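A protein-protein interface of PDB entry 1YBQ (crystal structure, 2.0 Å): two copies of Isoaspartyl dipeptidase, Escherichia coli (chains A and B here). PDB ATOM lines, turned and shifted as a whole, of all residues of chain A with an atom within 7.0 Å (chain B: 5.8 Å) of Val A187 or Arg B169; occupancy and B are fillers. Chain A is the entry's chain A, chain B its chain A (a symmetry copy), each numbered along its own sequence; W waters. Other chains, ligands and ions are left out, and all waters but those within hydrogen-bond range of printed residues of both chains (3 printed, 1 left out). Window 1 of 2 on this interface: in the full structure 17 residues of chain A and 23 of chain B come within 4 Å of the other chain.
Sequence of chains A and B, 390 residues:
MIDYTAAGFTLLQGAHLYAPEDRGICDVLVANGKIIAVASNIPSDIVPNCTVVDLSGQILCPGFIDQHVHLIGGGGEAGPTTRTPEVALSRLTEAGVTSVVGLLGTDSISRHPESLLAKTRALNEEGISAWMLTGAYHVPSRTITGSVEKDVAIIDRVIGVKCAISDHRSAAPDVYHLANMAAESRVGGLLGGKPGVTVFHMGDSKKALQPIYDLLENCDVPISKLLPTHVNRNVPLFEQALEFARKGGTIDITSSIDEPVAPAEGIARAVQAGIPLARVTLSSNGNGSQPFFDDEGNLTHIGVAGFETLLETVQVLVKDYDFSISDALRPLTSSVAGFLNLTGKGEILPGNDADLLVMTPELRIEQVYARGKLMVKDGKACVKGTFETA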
ATOM      1  N   GLU A 149      25.150  25.832   7.864  1.00  0.00           N
ATOM      2  CA  GLU A 149      24.755  24.428   8.034  1.00  0.00           C
ATOM      3  C   GLU A 149      25.973  23.513   8.186  1.00  0.00           C
ATOM      4  O   GLU A 149      26.033  22.665   9.065  1.00  0.00           O
ATOM      5  CB  GLU A 149      23.930  24.009   6.802  1.00  0.00           C
ATOM      6  CG  GLU A 149      23.138  22.701   6.933  1.00  0.00           C
ATOM      7  CD  GLU A 149      22.305  22.420   5.696  1.00  0.00           C
ATOM      8  OE1 GLU A 149      22.627  21.678   4.776  1.00  0.00           O
ATOM      9  OE2 GLU A 149      21.163  23.056   5.726  1.00  0.00           O
ATOM     10  N   VAL A 152      27.841  24.098  11.651  1.00  0.00           N
ATOM     11  CA  VAL A 152      27.128  23.484  12.755  1.00  0.00           C
ATOM     12  C   VAL A 152      27.155  21.972  12.604  1.00  0.00           C
ATOM     13  O   VAL A 152      27.271  21.204  13.545  1.00  0.00           O
ATOM     14  CB  VAL A 152      25.668  23.939  12.745  1.00  0.00           C
ATOM     15  CG1 VAL A 152      24.945  23.240  13.881  1.00  0.00           C
ATOM     16  CG2 VAL A 152      25.620  25.451  12.972  1.00  0.00           C
ATOM     17  N   ALA A 153      27.050  21.537  11.379  1.00  0.00           N
ATOM     18  CA  ALA A 153      27.045  20.131  11.190  1.00  0.00           C
ATOM     19  C   ALA A 153      28.423  19.518  11.376  1.00  0.00           C
ATOM     20  O   ALA A 153      28.570  18.451  11.954  1.00  0.00           O
ATOM     21  CB  ALA A 153      26.540  19.802   9.799  1.00  0.00           C
ATOM     22  N   ALA A 182      18.776  30.704  10.037  1.00  0.00           N
ATOM     23  CA  ALA A 182      18.190  29.926  11.110  1.00  0.00           C
ATOM     24  C   ALA A 182      17.939  28.457  10.718  1.00  0.00           C
ATOM     25  O   ALA A 182      18.159  27.484  11.470  1.00  0.00           O
ATOM     26  CB  ALA A 182      16.865  30.589  11.510  1.00  0.00           C
ATOM     27  N   ALA A 183      17.415  28.326   9.508  1.00  0.00           N
ATOM     28  CA  ALA A 183      17.083  27.044   8.950  1.00  0.00           C
ATOM     29  C   ALA A 183      18.346  26.183   8.800  1.00  0.00           C
ATOM     30  O   ALA A 183      18.363  24.987   9.089  1.00  0.00           O
ATOM     31  CB  ALA A 183      16.371  27.288   7.630  1.00  0.00           C
ATOM     32  N   GLU A 184      19.427  26.848   8.365  1.00  0.00           N
ATOM     33  CA  GLU A 184      20.701  26.153   8.179  1.00  0.00           C
ATOM     34  C   GLU A 184      21.259  25.678   9.498  1.00  0.00           C
ATOM     35  O   GLU A 184      21.868  24.618   9.577  1.00  0.00           O
ATOM     36  CB  GLU A 184      21.702  27.151   7.610  1.00  0.00           C
ATOM     37  CG  GLU A 184      21.425  27.282   6.115  1.00  0.00           C
ATOM     38  CD  GLU A 184      22.692  27.416   5.324  1.00  0.00           C
ATOM     39  OE1 GLU A 184      23.801  27.547   5.789  1.00  0.00           O
ATOM     40  OE2 GLU A 184      22.468  27.405   4.059  1.00  0.00           O
ATOM     41  N   SER A 185      21.084  26.527  10.529  1.00  0.00           N
ATOM     42  CA  SER A 185      21.592  26.144  11.845  1.00  0.00           C
ATOM     43  C   SER A 185      20.798  24.946  12.317  1.00  0.00           C
ATOM     44  O   SER A 185      21.356  23.972  12.830  1.00  0.00           O
ATOM     45  CB  SER A 185      21.474  27.233  12.899  1.00  0.00           C
ATOM     46  OG  SER A 185      22.137  26.807  14.072  1.00  0.00           O
ATOM     47  N   ARG A 186      19.479  25.068  12.133  1.00  0.00           N
ATOM     48  CA  ARG A 186      18.554  24.030  12.542  1.00  0.00           C
ATOM     49  C   ARG A 186      18.942  22.681  11.957  1.00  0.00           C
ATOM     50  O   ARG A 186      19.115  21.657  12.649  1.00  0.00           O
ATOM     51  CB  ARG A 186      17.125  24.413  12.150  1.00  0.00           C
ATOM     52  CG  ARG A 186      16.037  23.534  12.808  1.00  0.00           C
ATOM     53  CD  ARG A 186      15.990  22.096  12.285  1.00  0.00           C
ATOM     54  NE  ARG A 186      14.755  21.386  12.636  1.00  0.00           N
ATOM     55  CZ  ARG A 186      14.486  20.776  13.792  1.00  0.00           C
ATOM     56  NH1 ARG A 186      15.327  20.731  14.807  1.00  0.00           N
ATOM     57  NH2 ARG A 186      13.319  20.191  13.957  1.00  0.00           N
ATOM     58  N   VAL A 187      19.058  22.699  10.642  1.00  0.00           N
ATOM     59  CA  VAL A 187      19.407  21.501   9.959  1.00  0.00           C
ATOM     60  C   VAL A 187      20.839  21.021  10.283  1.00  0.00           C
ATOM     61  O   VAL A 187      21.061  19.829  10.504  1.00  0.00           O
ATOM     62  CB  VAL A 187      19.085  21.610   8.475  1.00  0.00           C
ATOM     63  CG1 VAL A 187      19.735  20.440   7.719  1.00  0.00           C
ATOM     64  CG2 VAL A 187      17.563  21.560   8.272  1.00  0.00           C
ATOM     65  N   GLY A 188      21.834  21.903  10.322  1.00  0.00           N
ATOM     66  CA  GLY A 188      23.183  21.424  10.625  1.00  0.00           C
ATOM     67  C   GLY A 188      23.223  20.814  12.024  1.00  0.00           C
ATOM     68  O   GLY A 188      24.040  19.954  12.328  1.00  0.00           O
ATOM     69  N   GLY A 189      22.323  21.265  12.894  1.00  0.00           N
ATOM     70  CA  GLY A 189      22.246  20.763  14.265  1.00  0.00           C
ATOM     71  C   GLY A 189      21.738  19.315  14.341  1.00  0.00           C
ATOM     72  O   GLY A 189      22.224  18.474  15.115  1.00  0.00           O
ATOM     73  N   LEU A 190      20.736  18.974  13.528  1.00  0.00           N
ATOM     74  CA  LEU A 190      20.240  17.598  13.563  1.00  0.00           C
ATOM     75  C   LEU A 190      21.348  16.633  13.108  1.00  0.00           C
ATOM     76  O   LEU A 190      21.591  15.564  13.616  1.00  0.00           O
ATOM     77  CB  LEU A 190      19.085  17.444  12.554  1.00  0.00           C
ATOM     78  CG  LEU A 190      17.805  18.230  12.932  1.00  0.00           C
ATOM     79  CD1 LEU A 190      16.768  18.135  11.815  1.00  0.00           C
ATOM     80  CD2 LEU A 190      17.184  17.725  14.226  1.00  0.00           C
ATOM     81  N   LEU A 191      21.999  17.039  12.063  1.00  0.00           N
ATOM     82  CA  LEU A 191      23.033  16.259  11.417  1.00  0.00           C
ATOM     83  C   LEU A 191      24.235  16.048  12.268  1.00  0.00           C
ATOM     84  O   LEU A 191      24.841  14.979  12.209  1.00  0.00           O
ATOM     85  CB  LEU A 191      23.577  16.918  10.116  1.00  0.00           C
ATOM     86  CG  LEU A 191      22.550  17.100   8.989  1.00  0.00           C
ATOM     87  CD1 LEU A 191      23.195  17.717   7.757  1.00  0.00           C
ATOM     88  CD2 LEU A 191      21.851  15.781   8.641  1.00  0.00           C
ATOM     89  N   GLY A 192      24.590  17.135  12.966  1.00  0.00           N
ATOM     90  CA  GLY A 192      25.764  17.159  13.816  1.00  0.00           C
ATOM     91  C   GLY A 192      25.437  16.806  15.257  1.00  0.00           C
ATOM     92  O   GLY A 192      26.326  16.556  16.086  1.00  0.00           O
ATOM     93  N   GLY A 193      24.153  16.755  15.571  1.00  0.00           N
ATOM     94  CA  GLY A 193      23.832  16.413  16.934  1.00  0.00           C
ATOM     95  C   GLY A 193      24.049  17.615  17.840  1.00  0.00           C
ATOM     96  O   GLY A 193      24.506  17.474  18.984  1.00  0.00           O
ATOM     97  N   GLY A 196      21.466  23.290  17.459  1.00  0.00           N
ATOM     98  CA  GLY A 196      21.208  24.061  16.237  1.00  0.00           C
ATOM     99  C   GLY A 196      20.427  25.357  16.502  1.00  0.00           C
ATOM    100  O   GLY A 196      19.424  25.652  15.868  1.00  0.00           O
ATOM    101  N   ASP A 220       9.962  27.222   8.892  1.00  0.00           N
ATOM    102  CA  ASP A 220       9.396  26.227   9.797  1.00  0.00           C
ATOM    103  C   ASP A 220      10.306  25.825  10.951  1.00  0.00           C
ATOM    104  O   ASP A 220      10.230  24.684  11.433  1.00  0.00           O
ATOM    105  CB  ASP A 220       8.771  25.038   9.034  1.00  0.00           C
ATOM    106  CG  ASP A 220       7.471  25.461   8.388  1.00  0.00           C
ATOM    107  OD1 ASP A 220       6.456  25.749   9.007  1.00  0.00           O
ATOM    108  OD2 ASP A 220       7.582  25.576   7.095  1.00  0.00           O
ATOM    109  N   VAL A 221      11.166  26.794  11.358  1.00  0.00           N
ATOM    110  CA  VAL A 221      12.099  26.635  12.470  1.00  0.00           C
ATOM    111  C   VAL A 221      11.292  26.774  13.750  1.00  0.00           C
ATOM    112  O   VAL A 221      10.527  27.742  13.917  1.00  0.00           O
ATOM    113  CB  VAL A 221      13.300  27.588  12.465  1.00  0.00           C
ATOM    114  CG1 VAL A 221      14.194  27.287  13.662  1.00  0.00           C
ATOM    115  CG2 VAL A 221      14.114  27.426  11.188  1.00  0.00           C
ATOM    116  N   GLU B  77      19.045  12.537  10.499  1.00  0.00           N
ATOM    117  CA  GLU B  77      18.345  13.442  11.427  1.00  0.00           C
ATOM    118  C   GLU B  77      18.678  13.319  12.906  1.00  0.00           C
ATOM    119  O   GLU B  77      18.332  14.158  13.726  1.00  0.00           O
ATOM    120  CB  GLU B  77      16.825  13.444  11.254  1.00  0.00           C
ATOM    121  CG  GLU B  77      16.432  13.993   9.896  1.00  0.00           C
ATOM    122  CD  GLU B  77      16.258  12.906   8.886  1.00  0.00           C
ATOM    123  OE1 GLU B  77      16.856  11.843   8.935  1.00  0.00           O
ATOM    124  OE2 GLU B  77      15.401  13.227   7.947  1.00  0.00           O
ATOM    125  N   THR B 106      17.320  15.009   3.541  1.00  0.00           N
ATOM    126  CA  THR B 106      17.749  15.992   4.500  1.00  0.00           C
ATOM    127  C   THR B 106      19.213  16.349   4.376  1.00  0.00           C
ATOM    128  O   THR B 106      19.613  17.505   4.287  1.00  0.00           O
ATOM    129  CB  THR B 106      17.417  15.519   5.930  1.00  0.00           C
ATOM    130  OG1 THR B 106      16.055  15.128   6.001  1.00  0.00           O
ATOM    131  CG2 THR B 106      17.621  16.657   6.909  1.00  0.00           C
ATOM    132  N   TYR B 137      17.129  18.613  -0.112  1.00  0.00           N
ATOM    133  CA  TYR B 137      16.160  19.415   0.613  1.00  0.00           C
ATOM    134  C   TYR B 137      16.592  20.839   0.479  1.00  0.00           C
ATOM    135  O   TYR B 137      15.794  21.738   0.244  1.00  0.00           O
ATOM    136  CB  TYR B 137      16.066  19.101   2.128  1.00  0.00           C
ATOM    137  CG  TYR B 137      15.152  17.955   2.617  1.00  0.00           C
ATOM    138  CD1 TYR B 137      14.805  16.853   1.824  1.00  0.00           C
ATOM    139  CD2 TYR B 137      14.684  17.967   3.936  1.00  0.00           C
ATOM    140  CE1 TYR B 137      13.999  15.819   2.309  1.00  0.00           C
ATOM    141  CE2 TYR B 137      13.877  16.949   4.448  1.00  0.00           C
ATOM    142  CZ  TYR B 137      13.546  15.867   3.632  1.00  0.00           C
ATOM    143  OH  TYR B 137      12.767  14.869   4.140  1.00  0.00           O
ATOM    144  N   ALA B 164      12.779  20.647  -0.658  1.00  0.00           N
ATOM    145  CA  ALA B 164      11.840  20.413   0.435  1.00  0.00           C
ATOM    146  C   ALA B 164      11.080  21.708   0.782  1.00  0.00           C
ATOM    147  O   ALA B 164      11.667  22.772   0.789  1.00  0.00           O
ATOM    148  CB  ALA B 164      12.611  19.894   1.640  1.00  0.00           C
ATOM    149  N   ASP B 167       8.279  22.395   5.740  1.00  0.00           N
ATOM    150  CA  ASP B 167       8.891  21.425   6.619  1.00  0.00           C
ATOM    151  C   ASP B 167       9.939  22.100   7.496  1.00  0.00           C
ATOM    152  O   ASP B 167      10.652  23.026   7.072  1.00  0.00           O
ATOM    153  CB  ASP B 167       9.463  20.282   5.728  1.00  0.00           C
ATOM    154  CG  ASP B 167      10.141  19.157   6.461  1.00  0.00           C
ATOM    155  OD1 ASP B 167      11.225  19.285   7.001  1.00  0.00           O
ATOM    156  OD2 ASP B 167       9.469  18.031   6.454  1.00  0.00           O
ATOM    157  N   HIS B 168       9.994  21.668   8.755  1.00  0.00           N
ATOM    158  CA  HIS B 168      10.927  22.253   9.700  1.00  0.00           C
ATOM    159  C   HIS B 168      12.383  21.948   9.348  1.00  0.00           C
ATOM    160  O   HIS B 168      13.276  22.359  10.073  1.00  0.00           O
ATOM    161  CB  HIS B 168      10.651  21.768  11.128  1.00  0.00           C
ATOM    162  CG  HIS B 168      10.683  20.259  11.249  1.00  0.00           C
ATOM    163  ND1 HIS B 168      11.882  19.541  11.393  1.00  0.00           N
ATOM    164  CD2 HIS B 168       9.655  19.355  11.259  1.00  0.00           C
ATOM    165  CE1 HIS B 168      11.561  18.253  11.471  1.00  0.00           C
ATOM    166  NE2 HIS B 168      10.233  18.105  11.386  1.00  0.00           N
ATOM    167  N   ARG B 169      12.631  21.221   8.253  1.00  0.00           N
ATOM    168  CA  ARG B 169      13.999  20.896   7.845  1.00  0.00           C
ATOM    169  C   ARG B 169      14.326  21.532   6.509  1.00  0.00           C
ATOM    170  O   ARG B 169      15.364  21.243   5.890  1.00  0.00           O
ATOM    171  CB  ARG B 169      14.307  19.395   7.807  1.00  0.00           C
ATOM    172  CG  ARG B 169      14.216  18.645   9.144  1.00  0.00           C
ATOM    173  CD  ARG B 169      13.933  17.126   8.950  1.00  0.00           C
ATOM    174  NE  ARG B 169      12.613  16.869   8.337  1.00  0.00           N
ATOM    175  CZ  ARG B 169      12.118  15.705   7.920  1.00  0.00           C
ATOM    176  NH1 ARG B 169      12.770  14.535   8.002  1.00  0.00           N
ATOM    177  NH2 ARG B 169      10.903  15.746   7.384  1.00  0.00           N
ATOM    178  N   SER B 170      13.434  22.414   6.040  1.00  0.00           N
ATOM    179  CA  SER B 170      13.677  23.110   4.764  1.00  0.00           C
ATOM    180  C   SER B 170      14.781  24.163   4.971  1.00  0.00           C
ATOM    181  O   SER B 170      15.203  24.434   6.092  1.00  0.00           O
ATOM    182  CB  SER B 170      12.429  23.872   4.329  1.00  0.00           C
ATOM    183  OG  SER B 170      12.403  25.089   5.098  1.00  0.00           O
ATOM    184  N   ALA B 171      15.229  24.771   3.896  1.00  0.00           N
ATOM    185  CA  ALA B 171      16.228  25.835   3.979  1.00  0.00           C
ATOM    186  C   ALA B 171      15.508  27.188   3.944  1.00  0.00           C
ATOM    187  O   ALA B 171      16.122  28.195   3.637  1.00  0.00           O
ATOM    188  CB  ALA B 171      17.335  25.747   2.921  1.00  0.00           C
ATOM    189  N   HIS B 201       9.440  17.718  -1.568  1.00  0.00           N
ATOM    190  CA  HIS B 201       9.174  16.955  -0.372  1.00  0.00           C
ATOM    191  C   HIS B 201       8.233  17.839   0.441  1.00  0.00           C
ATOM    192  O   HIS B 201       8.487  19.009   0.577  1.00  0.00           O
ATOM    193  CB  HIS B 201      10.436  16.652   0.478  1.00  0.00           C
ATOM    194  CG  HIS B 201      10.178  16.563   1.962  1.00  0.00           C
ATOM    195  ND1 HIS B 201      10.185  15.348   2.639  1.00  0.00           N
ATOM    196  CD2 HIS B 201       9.928  17.545   2.878  1.00  0.00           C
ATOM    197  CE1 HIS B 201       9.945  15.613   3.920  1.00  0.00           C
ATOM    198  NE2 HIS B 201       9.777  16.921   4.096  1.00  0.00           N
ATOM    199  N   GLY B 203       6.425  18.649   4.097  1.00  0.00           N
ATOM    200  CA  GLY B 203       6.532  18.387   5.490  1.00  0.00           C
ATOM    201  C   GLY B 203       5.130  18.614   6.045  1.00  0.00           C
ATOM    202  O   GLY B 203       4.137  18.705   5.297  1.00  0.00           O
ATOM    203  N   ARG B 233       0.859  12.329   4.277  1.00  0.00           N
ATOM    204  CA  ARG B 233       1.447  12.528   5.590  1.00  0.00           C
ATOM    205  C   ARG B 233       0.532  13.184   6.590  1.00  0.00           C
ATOM    206  O   ARG B 233       0.712  13.019   7.806  1.00  0.00           O
ATOM    207  CB  ARG B 233       2.816  13.185   5.553  1.00  0.00           C
ATOM    208  CG  ARG B 233       2.812  14.611   4.990  1.00  0.00           C
ATOM    209  CD  ARG B 233       4.189  15.245   5.130  1.00  0.00           C
ATOM    210  NE  ARG B 233       4.858  14.876   6.389  1.00  0.00           N
ATOM    211  CZ  ARG B 233       6.125  14.445   6.537  1.00  0.00           C
ATOM    212  NH1 ARG B 233       6.972  14.332   5.503  1.00  0.00           N
ATOM    213  NH2 ARG B 233       6.550  14.132   7.765  1.00  0.00           N
ATOM    214  N   SER B 289      15.187   7.552   5.851  1.00  0.00           N
ATOM    215  CA  SER B 289      14.817   7.377   7.227  1.00  0.00           C
ATOM    216  C   SER B 289      13.339   7.789   7.402  1.00  0.00           C
ATOM    217  O   SER B 289      12.707   8.545   6.632  1.00  0.00           O
ATOM    218  CB  SER B 289      15.708   8.174   8.181  1.00  0.00           C
ATOM    219  OG  SER B 289      15.417   9.556   8.024  1.00  0.00           O
ATOM    220  N   PRO B 291      11.745   9.440  10.280  1.00  0.00           N
ATOM    221  CA  PRO B 291      11.874  10.177  11.523  1.00  0.00           C
ATOM    222  C   PRO B 291      10.558  10.839  11.905  1.00  0.00           C
ATOM    223  O   PRO B 291       9.776  11.337  11.075  1.00  0.00           O
ATOM    224  CB  PRO B 291      12.958  11.237  11.276  1.00  0.00           C
ATOM    225  CG  PRO B 291      13.117  11.337   9.755  1.00  0.00           C
ATOM    226  CD  PRO B 291      12.323  10.197   9.131  1.00  0.00           C
ATOM    227  N   PHE B 293       8.802  13.642  14.488  1.00  0.00           N
ATOM    228  CA  PHE B 293       9.172  14.729  15.333  1.00  0.00           C
ATOM    229  C   PHE B 293       8.063  15.182  16.249  1.00  0.00           C
ATOM    230  O   PHE B 293       6.872  15.038  15.956  1.00  0.00           O
ATOM    231  CB  PHE B 293       9.760  15.902  14.523  1.00  0.00           C
ATOM    232  CG  PHE B 293      11.032  15.618  13.753  1.00  0.00           C
ATOM    233  CD1 PHE B 293      11.040  14.963  12.519  1.00  0.00           C
ATOM    234  CD2 PHE B 293      12.256  16.071  14.249  1.00  0.00           C
ATOM    235  CE1 PHE B 293      12.231  14.749  11.816  1.00  0.00           C
ATOM    236  CE2 PHE B 293      13.455  15.868  13.559  1.00  0.00           C
ATOM    237  CZ  PHE B 293      13.447  15.201  12.332  1.00  0.00           C
HETATM  238  O   HOH W   1      12.236  26.037   7.756  1.00  0.00           O
HETATM  239  O   HOH W   2       9.901  25.665   5.370  1.00  0.00           O
HETATM  240  O   HOH W   3      22.130  19.059   4.523  1.00  0.00           O
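A ring nitrogen (ND1) of His B168 is in hydrogen-bond range of the guanidinium group (NH2) of Arg A186 (3.0 Å).
No position is printed for both chains.
Of the 8 pairs that touch across the chains among the printed residues, none has its exchanged pair printed and touching as well.
Ser B170 touches Ala A183.
C of Ala B171 touches CB of Ala A183, at 3.8 Å.
Val A187 touches Arg B169 (CG2 to O, 3.3 Å).
Glu B77 touches Leu A190 (O to O, 3.6 Å).
Arg B169 touches Leu A190.
CB of Asp A220 touches O of Asp B167, at 3.4 Å.
His B168 touches Asp A220 (CB to O, 3.0 Å).
Water W2 lies within hydrogen-bond range of OG of Ser B170 (2.6 Å), OD2 of Asp A220 (2.9 Å) and O of Asp B167 (3.2 Å).
Water W3 bridges the side-chain carboxylate of Glu A149 (2.7 Å) and the backbone carbonyl oxygen of Thr B106 (3.0 Å).
Water W1 lies within hydrogen-bond range of N of Asp A220 (2.8 Å), OG of Ser B170 (2.8 Å) and O of Asp B167 (3.5 Å).
Hydrophobic or aromatic side chains of chain B within 4 Å of the printed part of chain A: His B168.
Of the 18 printed residues of chain A, 5 touch a printed residue of chain B.
Hydrophobic or aromatic side chains of chain A that line the printed part of chain B: Ala A183, Val A187 and Leu A190.
The side-chain carboxylate (OE2) of Glu B77 lies within hydrogen-bond range of the side-chain hydroxyl (OG1) of Thr B106 (2.8 Å).
The side-chain carboxylate (OE2) of Glu B77 is in salt-bridge range of the guanidinium group (NH1) of Arg B169.
The side-chain carboxylate of Glu B77 sits at hydrogen-bond distance from the side-chain hydroxyl of Ser B289 (2.9 Å).
The guanidinium group of Arg B169 lies within salt-bridge range of the side-chain carboxylate of Asp B167 (2.9 Å).
O of Asp B167 sits at hydrogen-bond distance from OG of Ser B170 (3.3 Å).
The side-chain carboxylate (OD2) of Asp B167 is in hydrogen-bond range of a ring nitrogen (NE2) of His B201, 2.6 Å away.
Of the printed residues of chain B, Ala A183 touches Ser B170 (3.4 Å) and Ala B171 (3.8 Å).
Of chain B, only Arg B169 comes within 4 Å of Val A187.
Of the printed residues of chain A, Asp B167 touches Asp A220.
Of chain A, only Val A187 and Leu A190 come within 4 Å of Arg B169.
Of the printed residues of chain A, Ser B170 touches Ala A183 (3.4 Å).
The nearest residue of chain A that does not touch Arg B169 is Arg A186 (4.5 Å).
The nearest printed residue of chain B that does not touch Asp A220 is Ser B170 (5.0 Å).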
